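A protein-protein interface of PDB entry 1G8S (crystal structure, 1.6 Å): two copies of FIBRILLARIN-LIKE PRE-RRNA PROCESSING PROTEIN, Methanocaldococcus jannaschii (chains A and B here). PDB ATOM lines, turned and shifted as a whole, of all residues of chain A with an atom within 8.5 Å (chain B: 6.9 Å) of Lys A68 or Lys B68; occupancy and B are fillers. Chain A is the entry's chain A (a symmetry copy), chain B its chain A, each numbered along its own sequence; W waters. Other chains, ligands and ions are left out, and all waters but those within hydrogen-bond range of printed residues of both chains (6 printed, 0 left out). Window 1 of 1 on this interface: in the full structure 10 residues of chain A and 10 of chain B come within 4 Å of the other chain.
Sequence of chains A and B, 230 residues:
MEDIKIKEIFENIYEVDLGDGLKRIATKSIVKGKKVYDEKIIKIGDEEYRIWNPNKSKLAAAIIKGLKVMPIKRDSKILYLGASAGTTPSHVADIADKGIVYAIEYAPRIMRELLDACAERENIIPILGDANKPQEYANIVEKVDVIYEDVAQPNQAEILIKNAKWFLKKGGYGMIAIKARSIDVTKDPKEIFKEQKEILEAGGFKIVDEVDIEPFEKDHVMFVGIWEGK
Among the printed residues, pairs that only touch across the chains: Lys A68 with Lys B68 (3.8 Å), Lys A68 with Val B208 (3.7 Å), Lys A68 with Asp B209 (3.4 Å), Val A208 with Lys B68 (3.7 Å) and Asp A209 with Lys B68 (3.4 Å).
N of Lys B68 is in hydrogen-bond range of OD1 of Asp B209, 2.8 Å away.
OD1 of Asp B209 lies within hydrogen-bond range of N of Val B69 (2.9 Å).
N of Lys A68 is in hydrogen-bond range of OD1 of Asp A209, at 2.8 Å.
The backbone NH of Val A69 sits at hydrogen-bond distance from the side-chain carboxylate of Asp A209 (2.9 Å).
The backbone NH of Val A208 sits at hydrogen-bond distance from the backbone carbonyl oxygen of Val A224 (2.8 Å).
The backbone carbonyl oxygen (O) of Asp A209 lies within hydrogen-bond range of the backbone NH (N) of Val A224 (3.0 Å).
Of the 20 printed residues of chain A, 3 touch a printed residue of chain B.
Among the printed residues, 5 pairs touch across the chains.
Among the printed residues, no Asp or Glu carboxylate lies within 4 Å of a Lys or Arg side-chain nitrogen of the other chain.
Lys B68 touches its own counterpart, Lys A68.
Lys A68 touches Val B208, and with the chains exchanged Val A208 touches Lys B68.
Lys A68 touches Asp B209, and with the chains exchanged Asp A209 touches Lys B68.
14 positions are printed for both chains.
Of the 5 pairs that touch across the chains among the printed residues, 5 have their exchanged pair printed and touching as well.
Lys B68 touches just these residues of chain A: Lys A68, Val A208 and Asp A209.
Printed residues of chain B within 4 Å of Val A208: Lys B68 (3.7 Å).
Printed residues of chain A within 4 Å of Asp B209: Lys A68.
Val A211 touches none of the printed residues of chain B.
The nearest residue of chain A that does not touch Lys B68 is Glu A210 (4.1 Å).
The nearest printed residue of chain B that does not touch Val A208 is Phe B10 (6.1 Å).
Water W6 lies within hydrogen-bond range of the backbone carbonyl oxygen of Val B208 (2.6 Å) and the backbone carbonyl oxygen of Lys A68 (2.7 Å).
Water W1 bridges O of Val A208 (2.6 Å) and O of Lys B68 (2.7 Å).
Water W2 lies within hydrogen-bond range of the backbone carbonyl oxygen (O) of Glu A210 (2.8 Å) and the side-chain amino group (NZ) of Lys B68 (2.9 Å).
Water W5 lies within hydrogen-bond range of the backbone carbonyl oxygen (O) of Glu B210 (2.8 Å) and the side-chain amino group (NZ) of Lys A68 (2.9 Å).
Water W3 bridges NZ of Lys A68 (2.8 Å) and N of Asp B209 (3.3 Å).
Water W4 bridges NZ of Lys B68 (2.8 Å) and N of Asp A209 (3.3 Å).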
ATOM      1  N   PHE A  10       7.407  -4.539 -20.112  1.00  0.00           N
ATOM      2  CA  PHE A  10       7.882  -3.837 -18.921  1.00  0.00           C
ATOM      3  C   PHE A  10       6.715  -2.984 -18.448  1.00  0.00           C
ATOM      4  O   PHE A  10       5.619  -3.501 -18.225  1.00  0.00           O
ATOM      5  CB  PHE A  10       9.093  -2.967 -19.267  1.00  0.00           C
ATOM      6  CG  PHE A  10      10.254  -3.749 -19.804  1.00  0.00           C
ATOM      7  CD1 PHE A  10      10.718  -3.532 -21.097  1.00  0.00           C
ATOM      8  CD2 PHE A  10      10.877  -4.722 -19.019  1.00  0.00           C
ATOM      9  CE1 PHE A  10      11.785  -4.271 -21.607  1.00  0.00           C
ATOM     10  CE2 PHE A  10      11.943  -5.464 -19.516  1.00  0.00           C
ATOM     11  CZ  PHE A  10      12.400  -5.242 -20.812  1.00  0.00           C
ATOM     12  N   LYS A  23      12.618  -6.680 -34.922  1.00  0.00           N
ATOM     13  CA  LYS A  23      12.279  -6.249 -33.572  1.00  0.00           C
ATOM     14  C   LYS A  23      12.241  -4.726 -33.505  1.00  0.00           C
ATOM     15  O   LYS A  23      13.179  -4.057 -33.939  1.00  0.00           O
ATOM     16  CB  LYS A  23      13.309  -6.783 -32.571  1.00  0.00           C
ATOM     17  CG  LYS A  23      13.384  -8.301 -32.519  1.00  0.00           C
ATOM     18  CD  LYS A  23      14.441  -8.779 -31.536  1.00  0.00           C
ATOM     19  CE  LYS A  23      14.533 -10.301 -31.527  1.00  0.00           C
ATOM     20  NZ  LYS A  23      15.596 -10.798 -30.605  1.00  0.00           N
ATOM     21  N   ALA A  62      19.796  -1.632 -25.650  1.00  0.00           N
ATOM     22  CA  ALA A  62      19.852  -2.631 -24.594  1.00  0.00           C
ATOM     23  C   ALA A  62      18.568  -3.465 -24.578  1.00  0.00           C
ATOM     24  O   ALA A  62      18.629  -4.685 -24.427  1.00  0.00           O
ATOM     25  CB  ALA A  62      20.050  -1.967 -23.244  1.00  0.00           C
ATOM     26  N   ILE A  63      17.424  -2.809 -24.754  1.00  0.00           N
ATOM     27  CA  ILE A  63      16.136  -3.506 -24.740  1.00  0.00           C
ATOM     28  C   ILE A  63      16.062  -4.442 -25.944  1.00  0.00           C
ATOM     29  O   ILE A  63      15.679  -5.612 -25.808  1.00  0.00           O
ATOM     30  CB  ILE A  63      14.959  -2.495 -24.754  1.00  0.00           C
ATOM     31  CG1 ILE A  63      14.903  -1.756 -23.408  1.00  0.00           C
ATOM     32  CG2 ILE A  63      13.624  -3.221 -25.011  1.00  0.00           C
ATOM     33  CD1 ILE A  63      13.928  -0.611 -23.360  1.00  0.00           C
ATOM     34  N   ILE A  64      16.446  -3.940 -27.113  1.00  0.00           N
ATOM     35  CA  ILE A  64      16.433  -4.748 -28.333  1.00  0.00           C
ATOM     36  C   ILE A  64      17.366  -5.951 -28.206  1.00  0.00           C
ATOM     37  O   ILE A  64      17.065  -7.042 -28.709  1.00  0.00           O
ATOM     38  CB  ILE A  64      16.865  -3.916 -29.566  1.00  0.00           C
ATOM     39  CG1 ILE A  64      15.801  -2.871 -29.890  1.00  0.00           C
ATOM     40  CG2 ILE A  64      17.117  -4.828 -30.761  1.00  0.00           C
ATOM     41  CD1 ILE A  64      14.472  -3.455 -30.352  1.00  0.00           C
ATOM     42  N   LYS A  65      18.491  -5.757 -27.523  1.00  0.00           N
ATOM     43  CA  LYS A  65      19.472  -6.810 -27.342  1.00  0.00           C
ATOM     44  C   LYS A  65      19.213  -7.762 -26.182  1.00  0.00           C
ATOM     45  O   LYS A  65      20.068  -8.592 -25.870  1.00  0.00           O
ATOM     46  CB  LYS A  65      20.876  -6.206 -27.211  1.00  0.00           C
ATOM     47  CG  LYS A  65      21.426  -5.640 -28.519  1.00  0.00           C
ATOM     48  CD  LYS A  65      21.458  -6.689 -29.647  1.00  0.00           C
ATOM     49  CE  LYS A  65      22.166  -7.980 -29.225  1.00  0.00           C
ATOM     50  NZ  LYS A  65      23.546  -7.758 -28.699  1.00  0.00           N
ATOM     51  N   GLY A  66      18.063  -7.635 -25.526  1.00  0.00           N
ATOM     52  CA  GLY A  66      17.745  -8.569 -24.455  1.00  0.00           C
ATOM     53  C   GLY A  66      17.671  -8.134 -23.003  1.00  0.00           C
ATOM     54  O   GLY A  66      17.641  -8.986 -22.112  1.00  0.00           O
ATOM     55  N   LEU A  67      17.650  -6.833 -22.736  1.00  0.00           N
ATOM     56  CA  LEU A  67      17.546  -6.374 -21.355  1.00  0.00           C
ATOM     57  C   LEU A  67      16.293  -6.985 -20.723  1.00  0.00           C
ATOM     58  O   LEU A  67      15.212  -6.956 -21.329  1.00  0.00           O
ATOM     59  CB  LEU A  67      17.426  -4.850 -21.311  1.00  0.00           C
ATOM     60  CG  LEU A  67      17.267  -4.187 -19.942  1.00  0.00           C
ATOM     61  CD1 LEU A  67      18.590  -4.196 -19.183  1.00  0.00           C
ATOM     62  CD2 LEU A  67      16.793  -2.761 -20.150  1.00  0.00           C
ATOM     63  N   LYS A  68      16.439  -7.524 -19.514  1.00  0.00           N
ATOM     64  CA  LYS A  68      15.322  -8.130 -18.792  1.00  0.00           C
ATOM     65  C   LYS A  68      14.940  -7.333 -17.551  1.00  0.00           C
ATOM     66  O   LYS A  68      13.813  -7.440 -17.063  1.00  0.00           O
ATOM     67  CB  LYS A  68      15.670  -9.569 -18.384  1.00  0.00           C
ATOM     68  CG  LYS A  68      16.036 -10.474 -19.552  1.00  0.00           C
ATOM     69  CD  LYS A  68      14.880 -10.658 -20.536  1.00  0.00           C
ATOM     70  CE  LYS A  68      15.321 -11.476 -21.728  1.00  0.00           C
ATOM     71  NZ  LYS A  68      14.299 -11.504 -22.809  1.00  0.00           N
ATOM     72  N   VAL A  69      15.877  -6.532 -17.029  1.00  0.00           N
ATOM     73  CA  VAL A  69      15.611  -5.726 -15.841  1.00  0.00           C
ATOM     74  C   VAL A  69      15.504  -4.256 -16.251  1.00  0.00           C
ATOM     75  O   VAL A  69      16.508  -3.619 -16.587  1.00  0.00           O
ATOM     76  CB  VAL A  69      16.743  -5.897 -14.785  1.00  0.00           C
ATOM     77  CG1 VAL A  69      16.379  -5.179 -13.502  1.00  0.00           C
ATOM     78  CG2 VAL A  69      16.977  -7.383 -14.508  1.00  0.00           C
ATOM     79  N   MET A  70      14.279  -3.737 -16.260  1.00  0.00           N
ATOM     80  CA  MET A  70      14.017  -2.347 -16.639  1.00  0.00           C
ATOM     81  C   MET A  70      13.263  -1.689 -15.486  1.00  0.00           C
ATOM     82  O   MET A  70      12.029  -1.748 -15.399  1.00  0.00           O
ATOM     83  CB  MET A  70      13.204  -2.300 -17.939  1.00  0.00           C
ATOM     84  CG  MET A  70      12.758  -0.908 -18.352  1.00  0.00           C
ATOM     85  SD  MET A  70      14.128   0.320 -18.366  1.00  0.00           S
ATOM     86  CE  MET A  70      13.346   1.595 -19.256  1.00  0.00           C
ATOM     87  N   PRO A  71      14.004  -1.039 -14.574  1.00  0.00           N
ATOM     88  CA  PRO A  71      13.472  -0.361 -13.390  1.00  0.00           C
ATOM     89  C   PRO A  71      12.708   0.943 -13.587  1.00  0.00           C
ATOM     90  O   PRO A  71      12.024   1.403 -12.671  1.00  0.00           O
ATOM     91  CB  PRO A  71      14.720  -0.163 -12.531  1.00  0.00           C
ATOM     92  CG  PRO A  71      15.751   0.122 -13.555  1.00  0.00           C
ATOM     93  CD  PRO A  71      15.475  -0.930 -14.619  1.00  0.00           C
ATOM     94  N   LYS A 197      32.726  -4.016 -13.505  1.00  0.00           N
ATOM     95  CA  LYS A 197      31.671  -4.686 -12.763  1.00  0.00           C
ATOM     96  C   LYS A 197      32.098  -4.800 -11.300  1.00  0.00           C
ATOM     97  O   LYS A 197      31.311  -4.529 -10.390  1.00  0.00           O
ATOM     98  CB  LYS A 197      31.427  -6.077 -13.357  1.00  0.00           C
ATOM     99  CG  LYS A 197      30.294  -6.852 -12.715  1.00  0.00           C
ATOM    100  CD  LYS A 197      30.134  -8.203 -13.397  1.00  0.00           C
ATOM    101  CE  LYS A 197      29.038  -9.029 -12.748  1.00  0.00           C
ATOM    102  NZ  LYS A 197      28.900 -10.360 -13.400  1.00  0.00           N
ATOM    103  N   ILE A 207      24.938  -6.423  -9.289  1.00  0.00           N
ATOM    104  CA  ILE A 207      24.609  -6.415 -10.713  1.00  0.00           C
ATOM    105  C   ILE A 207      23.528  -7.445 -11.035  1.00  0.00           C
ATOM    106  O   ILE A 207      23.697  -8.629 -10.747  1.00  0.00           O
ATOM    107  CB  ILE A 207      25.857  -6.704 -11.571  1.00  0.00           C
ATOM    108  CG1 ILE A 207      26.941  -5.659 -11.269  1.00  0.00           C
ATOM    109  CG2 ILE A 207      25.484  -6.697 -13.051  1.00  0.00           C
ATOM    110  CD1 ILE A 207      26.472  -4.231 -11.409  1.00  0.00           C
ATOM    111  N   VAL A 208      22.423  -6.985 -11.620  1.00  0.00           N
ATOM    112  CA  VAL A 208      21.313  -7.882 -11.960  1.00  0.00           C
ATOM    113  C   VAL A 208      21.046  -8.045 -13.459  1.00  0.00           C
ATOM    114  O   VAL A 208      20.204  -8.855 -13.860  1.00  0.00           O
ATOM    115  CB  VAL A 208      20.003  -7.466 -11.233  1.00  0.00           C
ATOM    116  CG1 VAL A 208      20.195  -7.600  -9.724  1.00  0.00           C
ATOM    117  CG2 VAL A 208      19.600  -6.049 -11.601  1.00  0.00           C
ATOM    118  N   ASP A 209      21.746  -7.274 -14.285  1.00  0.00           N
ATOM    119  CA  ASP A 209      21.621  -7.400 -15.734  1.00  0.00           C
ATOM    120  C   ASP A 209      22.864  -6.825 -16.404  1.00  0.00           C
ATOM    121  O   ASP A 209      23.539  -5.935 -15.860  1.00  0.00           O
ATOM    122  CB  ASP A 209      20.344  -6.724 -16.255  1.00  0.00           C
ATOM    123  CG  ASP A 209      19.789  -7.409 -17.511  1.00  0.00           C
ATOM    124  OD1 ASP A 209      18.600  -7.202 -17.826  1.00  0.00           O
ATOM    125  OD2 ASP A 209      20.538  -8.142 -18.189  1.00  0.00           O
ATOM    126  N   GLU A 210      23.179  -7.362 -17.574  1.00  0.00           N
ATOM    127  CA  GLU A 210      24.347  -6.953 -18.343  1.00  0.00           C
ATOM    128  C   GLU A 210      24.016  -7.240 -19.794  1.00  0.00           C
ATOM    129  O   GLU A 210      23.776  -8.391 -20.163  1.00  0.00           O
ATOM    130  CB  GLU A 210      25.567  -7.769 -17.913  1.00  0.00           C
ATOM    131  CG  GLU A 210      26.888  -7.276 -18.487  1.00  0.00           C
ATOM    132  CD  GLU A 210      28.068  -8.140 -18.064  1.00  0.00           C
ATOM    133  OE1 GLU A 210      28.142  -8.508 -16.874  1.00  0.00           O
ATOM    134  OE2 GLU A 210      28.923  -8.442 -18.922  1.00  0.00           O
ATOM    135  N   VAL A 211      24.010  -6.199 -20.619  1.00  0.00           N
ATOM    136  CA  VAL A 211      23.666  -6.347 -22.026  1.00  0.00           C
ATOM    137  C   VAL A 211      24.709  -5.767 -22.976  1.00  0.00           C
ATOM    138  O   VAL A 211      25.014  -4.567 -22.915  1.00  0.00           O
ATOM    139  CB  VAL A 211      22.317  -5.645 -22.328  1.00  0.00           C
ATOM    140  CG1 VAL A 211      21.853  -5.974 -23.754  1.00  0.00           C
ATOM    141  CG2 VAL A 211      21.271  -6.042 -21.282  1.00  0.00           C
ATOM    142  N   MET A 222      25.627  -2.405 -21.246  1.00  0.00           N
ATOM    143  CA  MET A 222      24.695  -1.759 -20.329  1.00  0.00           C
ATOM    144  C   MET A 222      24.626  -2.610 -19.069  1.00  0.00           C
ATOM    145  O   MET A 222      24.259  -3.792 -19.125  1.00  0.00           O
ATOM    146  CB  MET A 222      23.294  -1.653 -20.959  1.00  0.00           C
ATOM    147  CG  MET A 222      22.232  -1.003 -20.074  1.00  0.00           C
ATOM    148  SD  MET A 222      22.425   0.809 -19.817  1.00  0.00           S
ATOM    149  CE  MET A 222      21.722   1.405 -21.288  1.00  0.00           C
ATOM    150  N   VAL A 224      23.079  -3.085 -15.137  1.00  0.00           N
ATOM    151  CA  VAL A 224      21.966  -2.680 -14.300  1.00  0.00           C
ATOM    152  C   VAL A 224      22.248  -3.281 -12.938  1.00  0.00           C
ATOM    153  O   VAL A 224      22.568  -4.470 -12.827  1.00  0.00           O
ATOM    154  CB  VAL A 224      20.601  -3.211 -14.821  1.00  0.00           C
ATOM    155  CG1 VAL A 224      19.494  -2.782 -13.890  1.00  0.00           C
ATOM    156  CG2 VAL A 224      20.333  -2.694 -16.216  1.00  0.00           C
ATOM    157  N   PHE B  10      21.585 -14.119  -7.370  1.00  0.00           N
ATOM    158  CA  PHE B  10      20.158 -14.322  -7.127  1.00  0.00           C
ATOM    159  C   PHE B  10      20.012 -14.487  -5.622  1.00  0.00           C
ATOM    160  O   PHE B  10      20.454 -13.627  -4.858  1.00  0.00           O
ATOM    161  CB  PHE B  10      19.668 -15.570  -7.866  1.00  0.00           C
ATOM    162  CG  PHE B  10      19.849 -15.491  -9.352  1.00  0.00           C
ATOM    163  CD1 PHE B  10      20.682 -16.388 -10.013  1.00  0.00           C
ATOM    164  CD2 PHE B  10      19.198 -14.503 -10.095  1.00  0.00           C
ATOM    165  CE1 PHE B  10      20.869 -16.306 -11.392  1.00  0.00           C
ATOM    166  CE2 PHE B  10      19.375 -14.412 -11.471  1.00  0.00           C
ATOM    167  CZ  PHE B  10      20.212 -15.313 -12.125  1.00  0.00           C
ATOM    168  N   ALA B  62      20.034 -22.706 -18.163  1.00  0.00           N
ATOM    169  CA  ALA B  62      19.407 -21.408 -18.359  1.00  0.00           C
ATOM    170  C   ALA B  62      20.200 -20.315 -17.634  1.00  0.00           C
ATOM    171  O   ALA B  62      20.405 -19.235 -18.187  1.00  0.00           O
ATOM    172  CB  ALA B  62      17.977 -21.425 -17.852  1.00  0.00           C
ATOM    173  N   ILE B  63      20.654 -20.610 -16.420  1.00  0.00           N
ATOM    174  CA  ILE B  63      21.410 -19.635 -15.631  1.00  0.00           C
ATOM    175  C   ILE B  63      22.742 -19.358 -16.323  1.00  0.00           C
ATOM    176  O   ILE B  63      23.139 -18.196 -16.481  1.00  0.00           O
ATOM    177  CB  ILE B  63      21.635 -20.147 -14.184  1.00  0.00           C
ATOM    178  CG1 ILE B  63      20.297 -20.156 -13.429  1.00  0.00           C
ATOM    179  CG2 ILE B  63      22.650 -19.253 -13.445  1.00  0.00           C
ATOM    180  CD1 ILE B  63      20.343 -20.813 -12.077  1.00  0.00           C
ATOM    181  N   GLY B  66      22.459 -17.065 -19.329  1.00  0.00           N
ATOM    182  CA  GLY B  66      21.962 -15.705 -19.174  1.00  0.00           C
ATOM    183  C   GLY B  66      20.633 -15.404 -18.509  1.00  0.00           C
ATOM    184  O   GLY B  66      20.140 -14.277 -18.613  1.00  0.00           O
ATOM    185  N   LEU B  67      20.030 -16.378 -17.837  1.00  0.00           N
ATOM    186  CA  LEU B  67      18.766 -16.120 -17.156  1.00  0.00           C
ATOM    187  C   LEU B  67      18.955 -14.951 -16.185  1.00  0.00           C
ATOM    188  O   LEU B  67      19.932 -14.926 -15.424  1.00  0.00           O
ATOM    189  CB  LEU B  67      18.330 -17.353 -16.363  1.00  0.00           C
ATOM    190  CG  LEU B  67      17.040 -17.256 -15.548  1.00  0.00           C
ATOM    191  CD1 LEU B  67      15.820 -17.302 -16.463  1.00  0.00           C
ATOM    192  CD2 LEU B  67      17.001 -18.413 -14.569  1.00  0.00           C
ATOM    193  N   LYS B  68      18.023 -14.000 -16.210  1.00  0.00           N
ATOM    194  CA  LYS B  68      18.075 -12.836 -15.328  1.00  0.00           C
ATOM    195  C   LYS B  68      16.951 -12.844 -14.299  1.00  0.00           C
ATOM    196  O   LYS B  68      17.059 -12.203 -13.252  1.00  0.00           O
ATOM    197  CB  LYS B  68      18.003 -11.542 -16.150  1.00  0.00           C
ATOM    198  CG  LYS B  68      19.103 -11.405 -17.193  1.00  0.00           C
ATOM    199  CD  LYS B  68      20.498 -11.347 -16.569  1.00  0.00           C
ATOM    200  CE  LYS B  68      21.561 -11.316 -17.643  1.00  0.00           C
ATOM    201  NZ  LYS B  68      22.933 -11.472 -17.090  1.00  0.00           N
ATOM    202  N   VAL B  69      15.862 -13.566 -14.592  1.00  0.00           N
ATOM    203  CA  VAL B  69      14.730 -13.639 -13.674  1.00  0.00           C
ATOM    204  C   VAL B  69      14.691 -15.032 -13.043  1.00  0.00           C
ATOM    205  O   VAL B  69      14.350 -16.017 -13.708  1.00  0.00           O
ATOM    206  CB  VAL B  69      13.390 -13.358 -14.416  1.00  0.00           C
ATOM    207  CG1 VAL B  69      12.245 -13.286 -13.426  1.00  0.00           C
ATOM    208  CG2 VAL B  69      13.491 -12.048 -15.199  1.00  0.00           C
ATOM    209  N   MET B  70      15.078 -15.112 -11.773  1.00  0.00           N
ATOM    210  CA  MET B  70      15.103 -16.378 -11.037  1.00  0.00           C
ATOM    211  C   MET B  70      14.258 -16.198  -9.780  1.00  0.00           C
ATOM    212  O   MET B  70      14.739 -15.745  -8.733  1.00  0.00           O
ATOM    213  CB  MET B  70      16.550 -16.757 -10.691  1.00  0.00           C
ATOM    214  CG  MET B  70      16.683 -17.985  -9.807  1.00  0.00           C
ATOM    215  SD  MET B  70      15.735 -19.434 -10.429  1.00  0.00           S
ATOM    216  CE  MET B  70      16.456 -20.677  -9.446  1.00  0.00           C
ATOM    217  N   PRO B  71      12.968 -16.559  -9.864  1.00  0.00           N
ATOM    218  CA  PRO B  71      11.992 -16.448  -8.777  1.00  0.00           C
ATOM    219  C   PRO B  71      12.108 -17.412  -7.601  1.00  0.00           C
ATOM    220  O   PRO B  71      11.491 -17.190  -6.559  1.00  0.00           O
ATOM    221  CB  PRO B  71      10.660 -16.602  -9.508  1.00  0.00           C
ATOM    222  CG  PRO B  71      10.997 -17.603 -10.545  1.00  0.00           C
ATOM    223  CD  PRO B  71      12.333 -17.106 -11.078  1.00  0.00           C
ATOM    224  N   ILE B 207       5.301 -12.888 -20.072  1.00  0.00           N
ATOM    225  CA  ILE B 207       6.653 -13.432 -20.189  1.00  0.00           C
ATOM    226  C   ILE B 207       7.702 -12.386 -19.819  1.00  0.00           C
ATOM    227  O   ILE B 207       7.733 -11.307 -20.410  1.00  0.00           O
ATOM    228  CB  ILE B 207       6.923 -13.939 -21.619  1.00  0.00           C
ATOM    229  CG1 ILE B 207       5.885 -15.008 -21.991  1.00  0.00           C
ATOM    230  CG2 ILE B 207       8.342 -14.494 -21.716  1.00  0.00           C
ATOM    231  CD1 ILE B 207       5.787 -16.139 -20.995  1.00  0.00           C
ATOM    232  N   VAL B 208       8.545 -12.708 -18.839  1.00  0.00           N
ATOM    233  CA  VAL B 208       9.583 -11.774 -18.391  1.00  0.00           C
ATOM    234  C   VAL B 208      11.021 -12.225 -18.657  1.00  0.00           C
ATOM    235  O   VAL B 208      11.969 -11.470 -18.416  1.00  0.00           O
ATOM    236  CB  VAL B 208       9.412 -11.414 -16.888  1.00  0.00           C
ATOM    237  CG1 VAL B 208       8.087 -10.685 -16.687  1.00  0.00           C
ATOM    238  CG2 VAL B 208       9.483 -12.656 -16.017  1.00  0.00           C
ATOM    239  N   ASP B 209      11.191 -13.452 -19.142  1.00  0.00           N
ATOM    240  CA  ASP B 209      12.514 -13.953 -19.499  1.00  0.00           C
ATOM    241  C   ASP B 209      12.372 -15.105 -20.487  1.00  0.00           C
ATOM    242  O   ASP B 209      11.352 -15.815 -20.512  1.00  0.00           O
ATOM    243  CB  ASP B 209      13.314 -14.380 -18.258  1.00  0.00           C
ATOM    244  CG  ASP B 209      14.826 -14.196 -18.445  1.00  0.00           C
ATOM    245  OD1 ASP B 209      15.551 -14.160 -17.430  1.00  0.00           O
ATOM    246  OD2 ASP B 209      15.292 -14.100 -19.598  1.00  0.00           O
ATOM    247  N   GLU B 210      13.388 -15.266 -21.322  1.00  0.00           N
ATOM    248  CA  GLU B 210      13.412 -16.299 -22.349  1.00  0.00           C
ATOM    249  C   GLU B 210      14.875 -16.606 -22.603  1.00  0.00           C
ATOM    250  O   GLU B 210      15.633 -15.726 -23.016  1.00  0.00           O
ATOM    251  CB  GLU B 210      12.756 -15.778 -23.629  1.00  0.00           C
ATOM    252  CG  GLU B 210      12.522 -16.842 -24.694  1.00  0.00           C
ATOM    253  CD  GLU B 210      11.905 -16.272 -25.963  1.00  0.00           C
ATOM    254  OE1 GLU B 210      10.969 -15.453 -25.855  1.00  0.00           O
ATOM    255  OE2 GLU B 210      12.350 -16.652 -27.066  1.00  0.00           O
ATOM    256  N   VAL B 211      15.271 -17.851 -22.366  1.00  0.00           N
ATOM    257  CA  VAL B 211      16.660 -18.251 -22.536  1.00  0.00           C
ATOM    258  C   VAL B 211      16.842 -19.473 -23.430  1.00  0.00           C
ATOM    259  O   VAL B 211      16.302 -20.550 -23.137  1.00  0.00           O
ATOM    260  CB  VAL B 211      17.297 -18.579 -21.160  1.00  0.00           C
ATOM    261  CG1 VAL B 211      18.809 -18.800 -21.314  1.00  0.00           C
ATOM    262  CG2 VAL B 211      16.981 -17.469 -20.154  1.00  0.00           C
HETATM  263  O   HOH W   1      19.301 -10.941 -12.550  1.00  0.00           O
HETATM  264  O   HOH W   2      24.351 -11.029 -19.572  1.00  0.00           O
HETATM  265  O   HOH W   3      11.629 -12.094 -22.082  1.00  0.00           O
HETATM  266  O   HOH W   4      23.654  -9.860 -14.879  1.00  0.00           O
HETATM  267  O   HOH W   5      15.660 -13.403 -24.514  1.00  0.00           O
HETATM  268  O   HOH W   6      11.866  -8.856 -18.209  1.00  0.00           O
